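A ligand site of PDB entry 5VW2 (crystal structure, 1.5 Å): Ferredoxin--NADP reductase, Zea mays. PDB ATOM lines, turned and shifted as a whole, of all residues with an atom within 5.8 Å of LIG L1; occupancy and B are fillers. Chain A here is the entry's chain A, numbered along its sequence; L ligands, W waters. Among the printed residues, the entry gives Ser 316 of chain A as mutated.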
ATOM      1  N   SER A  71      -5.208   3.953  14.291  1.00  0.00           N
ATOM      2  CA  SER A  71      -4.064   4.691  14.764  1.00  0.00           C
ATOM      3  C   SER A  71      -3.801   5.892  13.869  1.00  0.00           C
ATOM      4  O   SER A  71      -4.098   5.867  12.683  1.00  0.00           O
ATOM      5  CB  SER A  71      -2.776   3.851  14.753  1.00  0.00           C
ATOM      6  OG  SER A  71      -2.870   2.739  15.620  1.00  0.00           O
ATOM      7  N   PRO A  76       7.607  13.124  14.207  1.00  0.00           N
ATOM      8  CA  PRO A  76       8.166  14.157  15.038  1.00  0.00           C
ATOM      9  C   PRO A  76       9.138  14.983  14.232  1.00  0.00           C
ATOM     10  O   PRO A  76       9.629  14.528  13.178  1.00  0.00           O
ATOM     11  CB  PRO A  76       8.868  13.366  16.144  1.00  0.00           C
ATOM     12  CG  PRO A  76       9.277  12.112  15.480  1.00  0.00           C
ATOM     13  CD  PRO A  76       8.149  11.796  14.542  1.00  0.00           C
ATOM     14  N   ARG A  91       5.813   7.384  14.019  1.00  0.00           N
ATOM     15  CA  ARG A  91       5.402   6.612  15.181  1.00  0.00           C
ATOM     16  C   ARG A  91       3.889   6.514  15.194  1.00  0.00           C
ATOM     17  O   ARG A  91       3.204   7.519  14.969  1.00  0.00           O
ATOM     18  CB  ARG A  91       5.840   7.259  16.491  1.00  0.00           C
ATOM     19  CG  ARG A  91       7.290   7.027  16.869  1.00  0.00           C
ATOM     20  CD  ARG A  91       8.288   7.792  16.029  1.00  0.00           C
ATOM     21  NE  ARG A  91       9.571   7.839  16.712  1.00  0.00           N
ATOM     22  CZ  ARG A  91      10.711   8.203  16.142  1.00  0.00           C
ATOM     23  NH1 ARG A  91      10.753   8.529  14.856  1.00  0.00           N
ATOM     24  NH2 ARG A  91      11.804   8.212  16.867  1.00  0.00           N
ATOM     25  N   LEU A  92       3.380   5.332  15.464  1.00  0.00           N
ATOM     26  CA  LEU A  92       1.946   5.139  15.509  1.00  0.00           C
ATOM     27  C   LEU A  92       1.403   5.325  16.925  1.00  0.00           C
ATOM     28  O   LEU A  92       2.019   4.911  17.901  1.00  0.00           O
ATOM     29  CB  LEU A  92       1.578   3.742  15.002  1.00  0.00           C
ATOM     30  CG  LEU A  92       1.901   3.490  13.538  1.00  0.00           C
ATOM     31  CD1 LEU A  92       1.728   2.019  13.218  1.00  0.00           C
ATOM     32  CD2 LEU A  92       0.983   4.322  12.664  1.00  0.00           C
ATOM     33  N   TYR A  93       0.225   5.938  17.019  1.00  0.00           N
ATOM     34  CA  TYR A  93      -0.464   6.113  18.283  1.00  0.00           C
ATOM     35  C   TYR A  93      -1.909   5.702  18.120  1.00  0.00           C
ATOM     36  O   TYR A  93      -2.585   6.140  17.180  1.00  0.00           O
ATOM     37  CB  TYR A  93      -0.343   7.546  18.827  1.00  0.00           C
ATOM     38  CG  TYR A  93       1.085   7.807  19.173  1.00  0.00           C
ATOM     39  CD1 TYR A  93       1.597   7.388  20.380  1.00  0.00           C
ATOM     40  CD2 TYR A  93       1.944   8.400  18.267  1.00  0.00           C
ATOM     41  CE1 TYR A  93       2.927   7.545  20.680  1.00  0.00           C
ATOM     42  CE2 TYR A  93       3.277   8.577  18.558  1.00  0.00           C
ATOM     43  CZ  TYR A  93       3.764   8.139  19.779  1.00  0.00           C
ATOM     44  OH  TYR A  93       5.105   8.286  20.072  1.00  0.00           O
ATOM     45  N   SER A  94      -2.370   4.874  19.031  1.00  0.00           N
ATOM     46  CA  SER A  94      -3.727   4.376  18.986  1.00  0.00           C
ATOM     47  C   SER A  94      -4.679   5.495  19.362  1.00  0.00           C
ATOM     48  O   SER A  94      -4.531   6.151  20.398  1.00  0.00           O
ATOM     49  CB  SER A  94      -3.856   3.237  19.978  1.00  0.00           C
ATOM     50  OG  SER A  94      -3.063   2.148  19.549  1.00  0.00           O
ATOM     51  N   ILE A  95      -5.662   5.740  18.518  1.00  0.00           N
ATOM     52  CA  ILE A  95      -6.557   6.866  18.796  1.00  0.00           C
ATOM     53  C   ILE A  95      -7.445   6.523  19.981  1.00  0.00           C
ATOM     54  O   ILE A  95      -8.057   5.438  20.037  1.00  0.00           O
ATOM     55  CB  ILE A  95      -7.337   7.231  17.529  1.00  0.00           C
ATOM     56  CG1 ILE A  95      -6.353   7.658  16.430  1.00  0.00           C
ATOM     57  CG2 ILE A  95      -8.303   8.351  17.839  1.00  0.00           C
ATOM     58  CD1 ILE A  95      -6.961   7.633  15.048  1.00  0.00           C
ATOM     59  N   CYS A 112      -3.199   8.906  23.755  1.00  0.00           N
ATOM     60  CA  CYS A 112      -2.872   8.558  25.129  1.00  0.00           C
ATOM     61  C   CYS A 112      -1.427   8.068  25.074  1.00  0.00           C
ATOM     62  O   CYS A 112      -1.156   6.972  24.578  1.00  0.00           O
ATOM     63  CB  CYS A 112      -3.810   7.451  25.584  1.00  0.00           C
ATOM     64  SG  CYS A 112      -3.535   6.873  27.216  1.00  0.00           S
ATOM     65  N   VAL A 113      -0.491   8.890  25.531  1.00  0.00           N
ATOM     66  CA  VAL A 113       0.919   8.735  25.183  1.00  0.00           C
ATOM     67  C   VAL A 113       1.753   8.586  26.452  1.00  0.00           C
ATOM     68  O   VAL A 113       1.743   9.464  27.319  1.00  0.00           O
ATOM     69  CB  VAL A 113       1.419   9.941  24.372  1.00  0.00           C
ATOM     70  CG1 VAL A 113       2.887   9.823  24.050  1.00  0.00           C
ATOM     71  CG2 VAL A 113       0.619  10.058  23.082  1.00  0.00           C
ATOM     72  N   ARG A 114       2.463   7.470  26.560  1.00  0.00           N
ATOM     73  CA  ARG A 114       3.429   7.284  27.636  1.00  0.00           C
ATOM     74  C   ARG A 114       4.748   7.917  27.235  1.00  0.00           C
ATOM     75  O   ARG A 114       5.285   7.619  26.160  1.00  0.00           O
ATOM     76  CB  ARG A 114       3.645   5.787  27.875  1.00  0.00           C
ATOM     77  CG  ARG A 114       4.745   5.473  28.885  1.00  0.00           C
ATOM     78  CD  ARG A 114       4.356   5.900  30.288  1.00  0.00           C
ATOM     79  NE  ARG A 114       5.441   5.688  31.262  1.00  0.00           N
ATOM     80  CZ  ARG A 114       5.644   4.569  31.949  1.00  0.00           C
ATOM     81  NH1 ARG A 114       6.670   4.502  32.792  1.00  0.00           N
ATOM     82  NH2 ARG A 114       4.835   3.518  31.818  1.00  0.00           N
ATOM     83  N   ALA A 116       8.391   7.995  26.930  1.00  0.00           N
ATOM     84  CA  ALA A 116       9.510   7.054  27.021  1.00  0.00           C
ATOM     85  C   ALA A 116      10.743   7.787  27.548  1.00  0.00           C
ATOM     86  O   ALA A 116      11.286   8.669  26.886  1.00  0.00           O
ATOM     87  CB  ALA A 116       9.772   6.435  25.659  1.00  0.00           C
ATOM     88  N   VAL A 117      11.187   7.402  28.747  1.00  0.00           N
ATOM     89  CA  VAL A 117      12.312   8.041  29.422  1.00  0.00           C
ATOM     90  C   VAL A 117      13.360   6.983  29.712  1.00  0.00           C
ATOM     91  O   VAL A 117      13.045   5.868  30.127  1.00  0.00           O
ATOM     92  CB  VAL A 117      11.838   8.714  30.737  1.00  0.00           C
ATOM     93  CG1 VAL A 117      13.004   9.339  31.486  1.00  0.00           C
ATOM     94  CG2 VAL A 117      10.804   9.771  30.430  1.00  0.00           C
ATOM     95  N   TYR A 118      14.611   7.338  29.461  1.00  0.00           N
ATOM     96  CA  TYR A 118      15.722   6.417  29.664  1.00  0.00           C
ATOM     97  C   TYR A 118      16.370   6.660  31.023  1.00  0.00           C
ATOM     98  O   TYR A 118      16.727   7.799  31.354  1.00  0.00           O
ATOM     99  CB  TYR A 118      16.772   6.619  28.575  1.00  0.00           C
ATOM    100  CG  TYR A 118      17.976   5.742  28.791  1.00  0.00           C
ATOM    101  CD1 TYR A 118      19.041   6.183  29.566  1.00  0.00           C
ATOM    102  CD2 TYR A 118      18.042   4.469  28.242  1.00  0.00           C
ATOM    103  CE1 TYR A 118      20.133   5.374  29.793  1.00  0.00           C
ATOM    104  CE2 TYR A 118      19.148   3.658  28.452  1.00  0.00           C
ATOM    105  CZ  TYR A 118      20.183   4.111  29.230  1.00  0.00           C
ATOM    106  OH  TYR A 118      21.285   3.331  29.459  1.00  0.00           O
ATOM    107  N   SER A 129      19.072  12.433  26.144  1.00  0.00           N
ATOM    108  CA  SER A 129      19.396  12.130  24.743  1.00  0.00           C
ATOM    109  C   SER A 129      18.911  10.749  24.329  1.00  0.00           C
ATOM    110  O   SER A 129      18.820  10.481  23.128  1.00  0.00           O
ATOM    111  CB  SER A 129      20.914  12.218  24.514  1.00  0.00           C
ATOM    112  OG  SER A 129      21.637  11.119  25.081  1.00  0.00           O
ATOM    113  N   LYS A 130      18.612   9.881  25.283  1.00  0.00           N
ATOM    114  CA  LYS A 130      18.112   8.551  24.978  1.00  0.00           C
ATOM    115  C   LYS A 130      16.626   8.430  25.236  1.00  0.00           C
ATOM    116  O   LYS A 130      16.075   7.332  25.174  1.00  0.00           O
ATOM    117  CB  LYS A 130      18.880   7.517  25.783  1.00  0.00           C
ATOM    118  CG  LYS A 130      20.351   7.539  25.440  1.00  0.00           C
ATOM    119  CD  LYS A 130      21.100   6.497  26.198  1.00  0.00           C
ATOM    120  CE  LYS A 130      22.575   6.568  25.855  1.00  0.00           C
ATOM    121  NZ  LYS A 130      23.368   5.603  26.656  1.00  0.00           N
ATOM    122  N   ASN A 131      15.963   9.541  25.534  1.00  0.00           N
ATOM    123  CA  ASN A 131      14.528   9.488  25.691  1.00  0.00           C
ATOM    124  C   ASN A 131      13.862   9.256  24.326  1.00  0.00           C
ATOM    125  O   ASN A 131      14.446   9.447  23.269  1.00  0.00           O
ATOM    126  CB  ASN A 131      14.019  10.768  26.349  1.00  0.00           C
ATOM    127  CG  ASN A 131      14.404  10.887  27.847  1.00  0.00           C
ATOM    128  OD1 ASN A 131      14.957   9.947  28.470  1.00  0.00           O
ATOM    129  ND2 ASN A 131      14.126  12.043  28.423  1.00  0.00           N
ATOM    130  N   GLY A 132      12.609   8.812  24.370  1.00  0.00           N
ATOM    131  CA  GLY A 132      11.866   8.604  23.140  1.00  0.00           C
ATOM    132  C   GLY A 132      11.523   9.941  22.486  1.00  0.00           C
ATOM    133  O   GLY A 132      11.043  10.869  23.145  1.00  0.00           O
ATOM    134  N   VAL A 133      11.792  10.042  21.190  1.00  0.00           N
ATOM    135  CA  VAL A 133      11.632  11.329  20.502  1.00  0.00           C
ATOM    136  C   VAL A 133      10.169  11.740  20.409  1.00  0.00           C
ATOM    137  O   VAL A 133       9.783  12.843  20.833  1.00  0.00           O
ATOM    138  CB  VAL A 133      12.289  11.286  19.115  1.00  0.00           C
ATOM    139  CG1 VAL A 133      12.027  12.599  18.348  1.00  0.00           C
ATOM    140  CG2 VAL A 133      13.770  11.024  19.253  1.00  0.00           C
ATOM    141  N   CYS A 134       9.324  10.873  19.832  1.00  0.00           N
ATOM    142  CA  CYS A 134       7.960  11.299  19.526  1.00  0.00           C
ATOM    143  C   CYS A 134       7.114  11.394  20.780  1.00  0.00           C
ATOM    144  O   CYS A 134       6.295  12.306  20.914  1.00  0.00           O
ATOM    145  CB  CYS A 134       7.341  10.351  18.513  1.00  0.00           C
ATOM    146  SG  CYS A 134       5.989  11.150  17.668  1.00  0.00           S
ATOM    147  N   SER A 135       7.300  10.476  21.729  1.00  0.00           N
ATOM    148  CA  SER A 135       6.439  10.512  22.907  1.00  0.00           C
ATOM    149  C   SER A 135       6.702  11.754  23.729  1.00  0.00           C
ATOM    150  O   SER A 135       5.769  12.390  24.230  1.00  0.00           O
ATOM    151  CB  SER A 135       6.591   9.236  23.748  1.00  0.00           C
ATOM    152  OG  SER A 135       7.925   9.081  24.228  1.00  0.00           O
ATOM    153  N   ASN A 136       7.976  12.125  23.899  1.00  0.00           N
ATOM    154  CA  ASN A 136       8.267  13.356  24.615  1.00  0.00           C
ATOM    155  C   ASN A 136       7.875  14.597  23.814  1.00  0.00           C
ATOM    156  O   ASN A 136       7.398  15.565  24.391  1.00  0.00           O
ATOM    157  CB  ASN A 136       9.725  13.374  25.065  1.00  0.00           C
ATOM    158  CG  ASN A 136       9.953  12.382  26.191  1.00  0.00           C
ATOM    159  OD1 ASN A 136       9.592  12.648  27.334  1.00  0.00           O
ATOM    160  ND2 ASN A 136      10.487  11.229  25.860  1.00  0.00           N
ATOM    161  N   THR A 175      -1.192   2.435  28.384  1.00  0.00           N
ATOM    162  CA  THR A 175      -1.785   3.189  27.287  1.00  0.00           C
ATOM    163  C   THR A 175      -2.455   2.304  26.249  1.00  0.00           C
ATOM    164  O   THR A 175      -3.132   2.821  25.370  1.00  0.00           O
ATOM    165  CB  THR A 175      -0.738   4.080  26.604  1.00  0.00           C
ATOM    166  OG1 THR A 175       0.365   3.293  26.171  1.00  0.00           O
ATOM    167  CG2 THR A 175      -0.270   5.158  27.555  1.00  0.00           C
ATOM    168  N   ALA A 178      -6.096   2.864  25.181  1.00  0.00           N
ATOM    169  CA  ALA A 178      -6.525   3.858  24.187  1.00  0.00           C
ATOM    170  C   ALA A 178      -7.723   3.466  23.334  1.00  0.00           C
ATOM    171  O   ALA A 178      -8.736   4.179  23.337  1.00  0.00           O
ATOM    172  CB  ALA A 178      -5.332   4.281  23.310  1.00  0.00           C
ATOM    173  N   GLU A 314      -3.399  -6.206  19.342  1.00  0.00           N
ATOM    174  CA  GLU A 314      -2.494  -5.167  18.837  1.00  0.00           C
ATOM    175  C   GLU A 314      -1.619  -4.746  20.007  1.00  0.00           C
ATOM    176  O   GLU A 314      -2.048  -4.003  20.899  1.00  0.00           O
ATOM    177  CB  GLU A 314      -3.284  -4.013  18.221  1.00  0.00           C
ATOM    178  CG  GLU A 314      -2.638  -3.464  16.938  1.00  0.00           C
ATOM    179  CD  GLU A 314      -3.382  -2.283  16.355  1.00  0.00           C
ATOM    180  OE1 GLU A 314      -3.441  -1.221  17.021  1.00  0.00           O
ATOM    181  OE2 GLU A 314      -3.909  -2.394  15.233  1.00  0.00           O
ATOM    182  N   VAL A 315      -0.395  -5.272  20.038  1.00  0.00           N
ATOM    183  CA  VAL A 315       0.526  -5.035  21.150  1.00  0.00           C
ATOM    184  C   VAL A 315       1.887  -4.754  20.546  1.00  0.00           C
ATOM    185  O   VAL A 315       2.160  -5.095  19.402  1.00  0.00           O
ATOM    186  CB  VAL A 315       0.609  -6.217  22.116  1.00  0.00           C
ATOM    187  CG1 VAL A 315      -0.734  -6.469  22.776  1.00  0.00           C
ATOM    188  CG2 VAL A 315       1.091  -7.485  21.409  1.00  0.00           C
ATOM    189  N   SER A 316       2.734  -4.109  21.334  1.00  0.00           N
ATOM    190  CA  SER A 316       4.072  -3.808  20.859  1.00  0.00           C
ATOM    191  C   SER A 316       4.997  -3.491  22.012  1.00  0.00           C
ATOM    192  O   SER A 316       4.603  -3.493  23.180  1.00  0.00           O
ATOM    193  CB  SER A 316       4.028  -2.628  19.903  1.00  0.00           C
ATOM    194  OG  SER A 316       3.562  -1.471  20.563  1.00  0.00           O
ATOM    195  OXT SER A 316       6.187  -3.212  21.777  1.00  0.00           O
HETATM  196  P1  LIG L   1      11.962   6.391  20.043  1.00  0.00           P
HETATM  197  O1  LIG L   1      11.474   5.647  18.856  1.00  0.00           O
HETATM  198  O2  LIG L   1      12.757   7.666  19.848  1.00  0.00           O
HETATM  199  O3  LIG L   1      12.837   5.401  20.959  1.00  0.00           O
HETATM  200  C1  LIG L   1      12.370   4.076  21.191  1.00  0.00           C
HETATM  201  C2  LIG L   1      12.840   3.628  22.552  1.00  0.00           C
HETATM  202  O4  LIG L   1      14.274   3.560  22.562  1.00  0.00           O
HETATM  203  C3  LIG L   1      12.496   4.595  23.682  1.00  0.00           C
HETATM  204  O5  LIG L   1      12.082   3.843  24.822  1.00  0.00           O
HETATM  205  C4  LIG L   1      13.787   5.325  23.986  1.00  0.00           C
HETATM  206  O6  LIG L   1      13.826   5.807  25.316  1.00  0.00           O
HETATM  207  C5  LIG L   1      14.779   4.234  23.703  1.00  0.00           C
HETATM  208  N1  LIG L   1      16.116   4.695  23.309  1.00  0.00           N
HETATM  209  C6  LIG L   1      16.424   5.643  22.418  1.00  0.00           C
HETATM  210  N2  LIG L   1      17.770   5.771  22.299  1.00  0.00           N
HETATM  211  C7  LIG L   1      18.312   4.862  23.125  1.00  0.00           C
HETATM  212  C8  LIG L   1      19.665   4.436  23.511  1.00  0.00           C
HETATM  213  N3  LIG L   1      20.708   5.056  22.933  1.00  0.00           N
HETATM  214  N4  LIG L   1      19.783   3.461  24.432  1.00  0.00           N
HETATM  215  C9  LIG L   1      18.723   2.852  24.995  1.00  0.00           C
HETATM  216  N5  LIG L   1      17.457   3.202  24.696  1.00  0.00           N
HETATM  217  C10 LIG L   1      17.229   4.173  23.797  1.00  0.00           C
HETATM  218  N6  LIG L   1       2.515   4.203  22.521  1.00  0.00           N
HETATM  219  C11 LIG L   1       1.763   4.926  23.338  1.00  0.00           C
HETATM  220  O7  LIG L   1       2.291   5.439  24.352  1.00  0.00           O
HETATM  221  N7  LIG L   1       0.455   5.098  23.112  1.00  0.00           N
HETATM  222  C12 LIG L   1      -0.180   4.562  22.059  1.00  0.00           C
HETATM  223  O8  LIG L   1      -1.397   4.758  21.847  1.00  0.00           O
HETATM  224  C13 LIG L   1       0.594   3.758  21.104  1.00  0.00           C
HETATM  225  N8  LIG L   1       0.026   3.148  20.059  1.00  0.00           N
HETATM  226  C14 LIG L   1       0.754   2.376  19.247  1.00  0.00           C
HETATM  227  C15 LIG L   1       0.136   1.678  18.211  1.00  0.00           C
HETATM  228  C16 LIG L   1       0.855   0.827  17.376  1.00  0.00           C
HETATM  229  C17 LIG L   1       0.180   0.064  16.263  1.00  0.00           C
HETATM  230  C18 LIG L   1       2.291   0.658  17.626  1.00  0.00           C
HETATM  231  C19 LIG L   1       3.115  -0.260  16.768  1.00  0.00           C
HETATM  232  C20 LIG L   1       2.904   1.346  18.640  1.00  0.00           C
HETATM  233  C21 LIG L   1       2.205   2.195  19.480  1.00  0.00           C
HETATM  234  N9  LIG L   1       2.814   2.883  20.545  1.00  0.00           N
HETATM  235  C22 LIG L   1       2.025   3.618  21.424  1.00  0.00           C
HETATM  236  C23 LIG L   1       4.274   3.054  20.632  1.00  0.00           C
HETATM  237  C24 LIG L   1       4.701   4.314  19.873  1.00  0.00           C
HETATM  238  O9  LIG L   1       4.436   4.128  18.490  1.00  0.00           O
HETATM  239  C25 LIG L   1       6.191   4.592  20.028  1.00  0.00           C
HETATM  240  O10 LIG L   1       6.961   3.465  19.635  1.00  0.00           O
HETATM  241  C26 LIG L   1       6.536   5.014  21.440  1.00  0.00           C
HETATM  242  O11 LIG L   1       5.789   6.180  21.756  1.00  0.00           O
HETATM  243  C27 LIG L   1       8.003   5.384  21.547  1.00  0.00           C
HETATM  244  O12 LIG L   1       8.316   6.263  20.462  1.00  0.00           O
HETATM  245  P2  LIG L   1       9.365   7.439  20.697  1.00  0.00           P
HETATM  246  O13 LIG L   1       9.528   8.158  19.398  1.00  0.00           O
HETATM  247  O14 LIG L   1       9.023   8.195  21.922  1.00  0.00           O
HETATM  248  O15 LIG L   1      10.749   6.651  21.074  1.00  0.00           O
HETATM  249  P1  LG2 L   2       3.503   0.323  31.819  1.00  0.00           P
HETATM  250  O1  LG2 L   2       3.295   1.181  33.037  1.00  0.00           O
HETATM  251  O2  LG2 L   2       4.919   0.029  31.339  1.00  0.00           O
HETATM  252  O3  LG2 L   2       2.777  -1.066  32.075  1.00  0.00           O
HETATM  253  C1  LG2 L   2       1.361  -1.140  32.237  1.00  0.00           C
HETATM  254  C2  LG2 L   2       1.092  -2.261  33.213  1.00  0.00           C
HETATM  255  O4  LG2 L   2       1.404  -3.540  32.637  1.00  0.00           O
HETATM  256  C3  LG2 L   2       1.982  -2.112  34.420  1.00  0.00           C
HETATM  257  O5  LG2 L   2       1.219  -2.382  35.586  1.00  0.00           O
HETATM  258  C4  LG2 L   2       3.039  -3.169  34.289  1.00  0.00           C
HETATM  259  O6  LG2 L   2       3.490  -3.584  35.572  1.00  0.00           O
HETATM  260  C5  LG2 L   2       2.217  -4.226  33.585  1.00  0.00           C
HETATM  261  N1  LG2 L   2       3.060  -5.256  32.982  1.00  0.00           N
HETATM  262  C6  LG2 L   2       4.396  -5.237  32.757  1.00  0.00           C
HETATM  263  N2  LG2 L   2       4.789  -6.410  32.212  1.00  0.00           N
HETATM  264  C7  LG2 L   2       3.688  -7.184  32.114  1.00  0.00           C
HETATM  265  C8  LG2 L   2       3.378  -8.545  31.632  1.00  0.00           C
HETATM  266  N3  LG2 L   2       4.373  -9.325  31.140  1.00  0.00           N
HETATM  267  N4  LG2 L   2       2.105  -8.958  31.722  1.00  0.00           N
HETATM  268  C9  LG2 L   2       1.122  -8.179  32.208  1.00  0.00           C
HETATM  269  N5  LG2 L   2       1.328  -6.932  32.663  1.00  0.00           N
HETATM  270  C10 LG2 L   2       2.571  -6.417  32.636  1.00  0.00           C
HETATM  271  O7  LG2 L   2       2.534   0.910  30.695  1.00  0.00           O
HETATM  272  P2  LG2 L   2       2.809   1.742  29.352  1.00  0.00           P
HETATM  273  O8  LG2 L   2       4.205   2.288  29.304  1.00  0.00           O
HETATM  274  O9  LG2 L   2       1.578   2.571  29.150  1.00  0.00           O
HETATM  275  O10 LG2 L   2       2.753   0.408  28.472  1.00  0.00           O
HETATM  276  C11 LG2 L   2       1.824   0.231  27.440  1.00  0.00           C
HETATM  277  C12 LG2 L   2       2.690  -0.086  26.257  1.00  0.00           C
HETATM  278  O11 LG2 L   2       1.872  -0.501  25.184  1.00  0.00           O
HETATM  279  C13 LG2 L   2       3.505   1.118  25.819  1.00  0.00           C
HETATM  280  O12 LG2 L   2       4.889   0.773  25.756  1.00  0.00           O
HETATM  281  C14 LG2 L   2       2.957   1.470  24.458  1.00  0.00           C
HETATM  282  O13 LG2 L   2       3.997   1.882  23.572  1.00  0.00           O
HETATM  283  C15 LG2 L   2       2.269   0.172  24.010  1.00  0.00           C
HETATM  284  N6  LG2 L   2       1.060   0.361  23.221  1.00  0.00           N
HETATM  285  C16 LG2 L   2       0.909  -0.365  22.102  1.00  0.00           C
HETATM  286  C17 LG2 L   2      -0.237  -0.220  21.340  1.00  0.00           C
HETATM  287  C18 LG2 L   2      -0.377  -1.016  20.080  1.00  0.00           C
HETATM  288  O14 LG2 L   2       0.537  -1.741  19.710  1.00  0.00           O
HETATM  289  N7  LG2 L   2      -1.473  -0.924  19.353  1.00  0.00           N
HETATM  290  C19 LG2 L   2      -1.214   0.680  21.753  1.00  0.00           C
HETATM  291  C20 LG2 L   2      -1.034   1.394  22.921  1.00  0.00           C
HETATM  292  C21 LG2 L   2       0.106   1.189  23.651  1.00  0.00           C
HETATM  293  P3  LG2 L   2       4.991  -3.309  36.113  1.00  0.00           P
HETATM  294  O15 LG2 L   2       5.714  -4.594  35.781  1.00  0.00           O
HETATM  295  O16 LG2 L   2       5.563  -2.127  35.373  1.00  0.00           O
HETATM  296  O17 LG2 L   2       4.688  -3.098  37.572  1.00  0.00           O
HETATM  297  O   HOH W   1      15.326   7.678  19.941  1.00  0.00           O
HETATM  298  O   HOH W   2      15.639   1.930  26.699  1.00  0.00           O
HETATM  299  O   HOH W   3      16.104   2.668  20.388  1.00  0.00           O
HETATM  300  O   HOH W   4      19.510   7.805  21.115  1.00  0.00           O
HETATM  301  O   HOH W   5       4.961   5.766  24.335  1.00  0.00           O
HETATM  302  O   HOH W   6      12.924   4.616  17.028  1.00  0.00           O
HETATM  303  O   HOH W   7       4.698  -1.433  13.901  1.00  0.00           O
HETATM  304  O   HOH W   8       9.252   3.190  24.003  1.00  0.00           O
HETATM  305  O   HOH W   9      19.960   1.512  21.675  1.00  0.00           O
HETATM  306  O   HOH W  10      23.362   3.477  23.418  1.00  0.00           O
HETATM  307  O   HOH W  11       6.507   0.558  19.524  1.00  0.00           O
HETATM  308  O   HOH W  12       5.484   3.245  16.140  1.00  0.00           O
HETATM  309  O   HOH W  13      22.189   3.085  25.935  1.00  0.00           O
HETATM  310  O   HOH W  14      12.818   4.402  27.754  1.00  0.00           O
HETATM  311  O   HOH W  15       9.448   3.799  18.554  1.00  0.00           O
HETATM  312  O   HOH W  16      -2.545   7.164  21.743  1.00  0.00           O
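The side-chain carboxylate (OE1) of Glu 314 lies within hydrogen-bond range of a nitrogen (N7) of LG2 L2, 3.1 Å away. The side-chain hydroxyl (OG) of Ser 94 is in hydrogen-bond range of a nitrogen (N8) of LIG L1 (3.3 Å). The backbone NH (N) of Ser 135 sits at hydrogen-bond distance from an oxygen (O14) of LIG L1 (2.9 Å). N7 of LG2 L2 lies within hydrogen-bond range of O of Glu 314 (3.5 Å). An oxygen (O13) of LIG L1 is in salt-bridge range of the guanidinium group of Arg 91, 2.7 Å away. A nitrogen (N7) of LG2 L2 lies close to the side-chain hydroxyl of Ser 94 (3.5 Å). The side-chain hydroxyl (OG) of Ser 316 lies within hydrogen-bond range of an oxygen (O14) of LG2 L2 (3.2 Å). A nitrogen (N7) of LIG L1 lies within hydrogen-bond range of the backbone carbonyl oxygen of Cys 112 (2.9 Å). An oxygen (O2) of LIG L1 sits at hydrogen-bond distance from the backbone NH (N) of Val 133 (2.9 Å). The backbone NH (N) of Cys 134 lies within hydrogen-bond range of an oxygen (O13) of LIG L1 (2.8 Å). The side-chain hydroxyl of Thr 175 sits at hydrogen-bond distance from an oxygen (O7) of LIG L1. The backbone NH (N) of Leu 92 is in hydrogen-bond range of an oxygen (O9) of LIG L1 (3.4 Å). The side-chain hydroxyl (OG) of Ser 135 is in hydrogen-bond range of an oxygen (O14) of LIG L1 (2.7 Å). O of Lys 130 lies within hydrogen-bond range of O6 of LIG L1 (2.7 Å). The backbone NH of Ser 94 sits at hydrogen-bond distance from an oxygen (O8) of LIG L1 (3.0 Å). O9 of LG2 L2 sits close to OG1 of Thr 175 (3.3 Å). The backbone carbonyl oxygen (O) of Leu 92 lies within hydrogen-bond range of an oxygen (O9) of LIG L1, at 2.6 Å. The backbone NH (N) of Thr 175 is in hydrogen-bond range of an oxygen (O9) of LG2 L2 (2.9 Å). An oxygen (O11) of LIG L1 is in hydrogen-bond range of the side-chain hydroxyl of Tyr 93, at 2.8 Å. NH2 of Arg 114 lies within salt-bridge range of O8 of LG2 L2, 2.9 Å away. The backbone NH (N) of Gly 132 lies within hydrogen-bond range of an oxygen (O6) of LIG L1 (3.4 Å). N of Arg 114 sits at hydrogen-bond distance from O7 of LIG L1.
A nitrogen (N6) of LIG L1 is in hydrogen-bond range of an oxygen (O13) of LG2 L2, 2.9 Å away.
OG of Ser 135 sits at hydrogen-bond distance from N of Ala 116 (2.9 Å). The backbone carbonyl oxygen (O) of Ala 116 lies within hydrogen-bond range of the side-chain amide nitrogen (ND2) of Asn 136, 2.9 Å away. The backbone NH of Tyr 118 is in hydrogen-bond range of the side-chain amide oxygen of Asn 131 (2.8 Å). The backbone carbonyl oxygen (O) of Gly 132 lies within hydrogen-bond range of the side-chain amide nitrogen (ND2) of Asn 136. The backbone NH (N) of Gly 132 lies within hydrogen-bond range of the backbone carbonyl oxygen (O) of Ala 116 (2.8 Å).
Val 113 touches LIG L1. Ala 116 touches LIG L1. CE2 of Tyr 118 touches C9 of LIG L1 (3.6 Å). C of Asn 131 touches O6 of LIG L1, at 3.6 Å. OE1 of Glu 314 touches C17 of LIG L1, at 3.9 Å. Ser 316 touches LIG L1 (OG to C20, 3.5 Å). Of the 26 residues printed, 18 come within 4 Å of LIG L1. The nearest printed residue that does not touch LIG L1 is Ser 71 (4.1 Å).
Water W16 lies within hydrogen-bond range of the backbone carbonyl oxygen of Ser 94 (2.6 Å), an oxygen (O8) of LIG L1 (2.7 Å) and the backbone NH of Cys 112 (2.7 Å). Water W5 lies within hydrogen-bond range of the backbone carbonyl oxygen of Arg 114 and an oxygen (O7) of LIG L1. Water W12 lies within hydrogen-bond range of an oxygen (O9) of LIG L1 (2.7 Å) and the backbone NH (N) of Leu 92 (3.0 Å). Water W13 lies within hydrogen-bond range of a nitrogen (N4) of LIG L1 (2.9 Å) and the side-chain amino group of Lys 130 (2.9 Å). Water W4 bridges a nitrogen (N2) of LIG L1 and the backbone carbonyl oxygen of Ser 129. Water W14 lies within hydrogen-bond range of the backbone carbonyl oxygen (O) of Val 117 (2.8 Å) and an oxygen (O6) of LIG L1 (3.0 Å).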
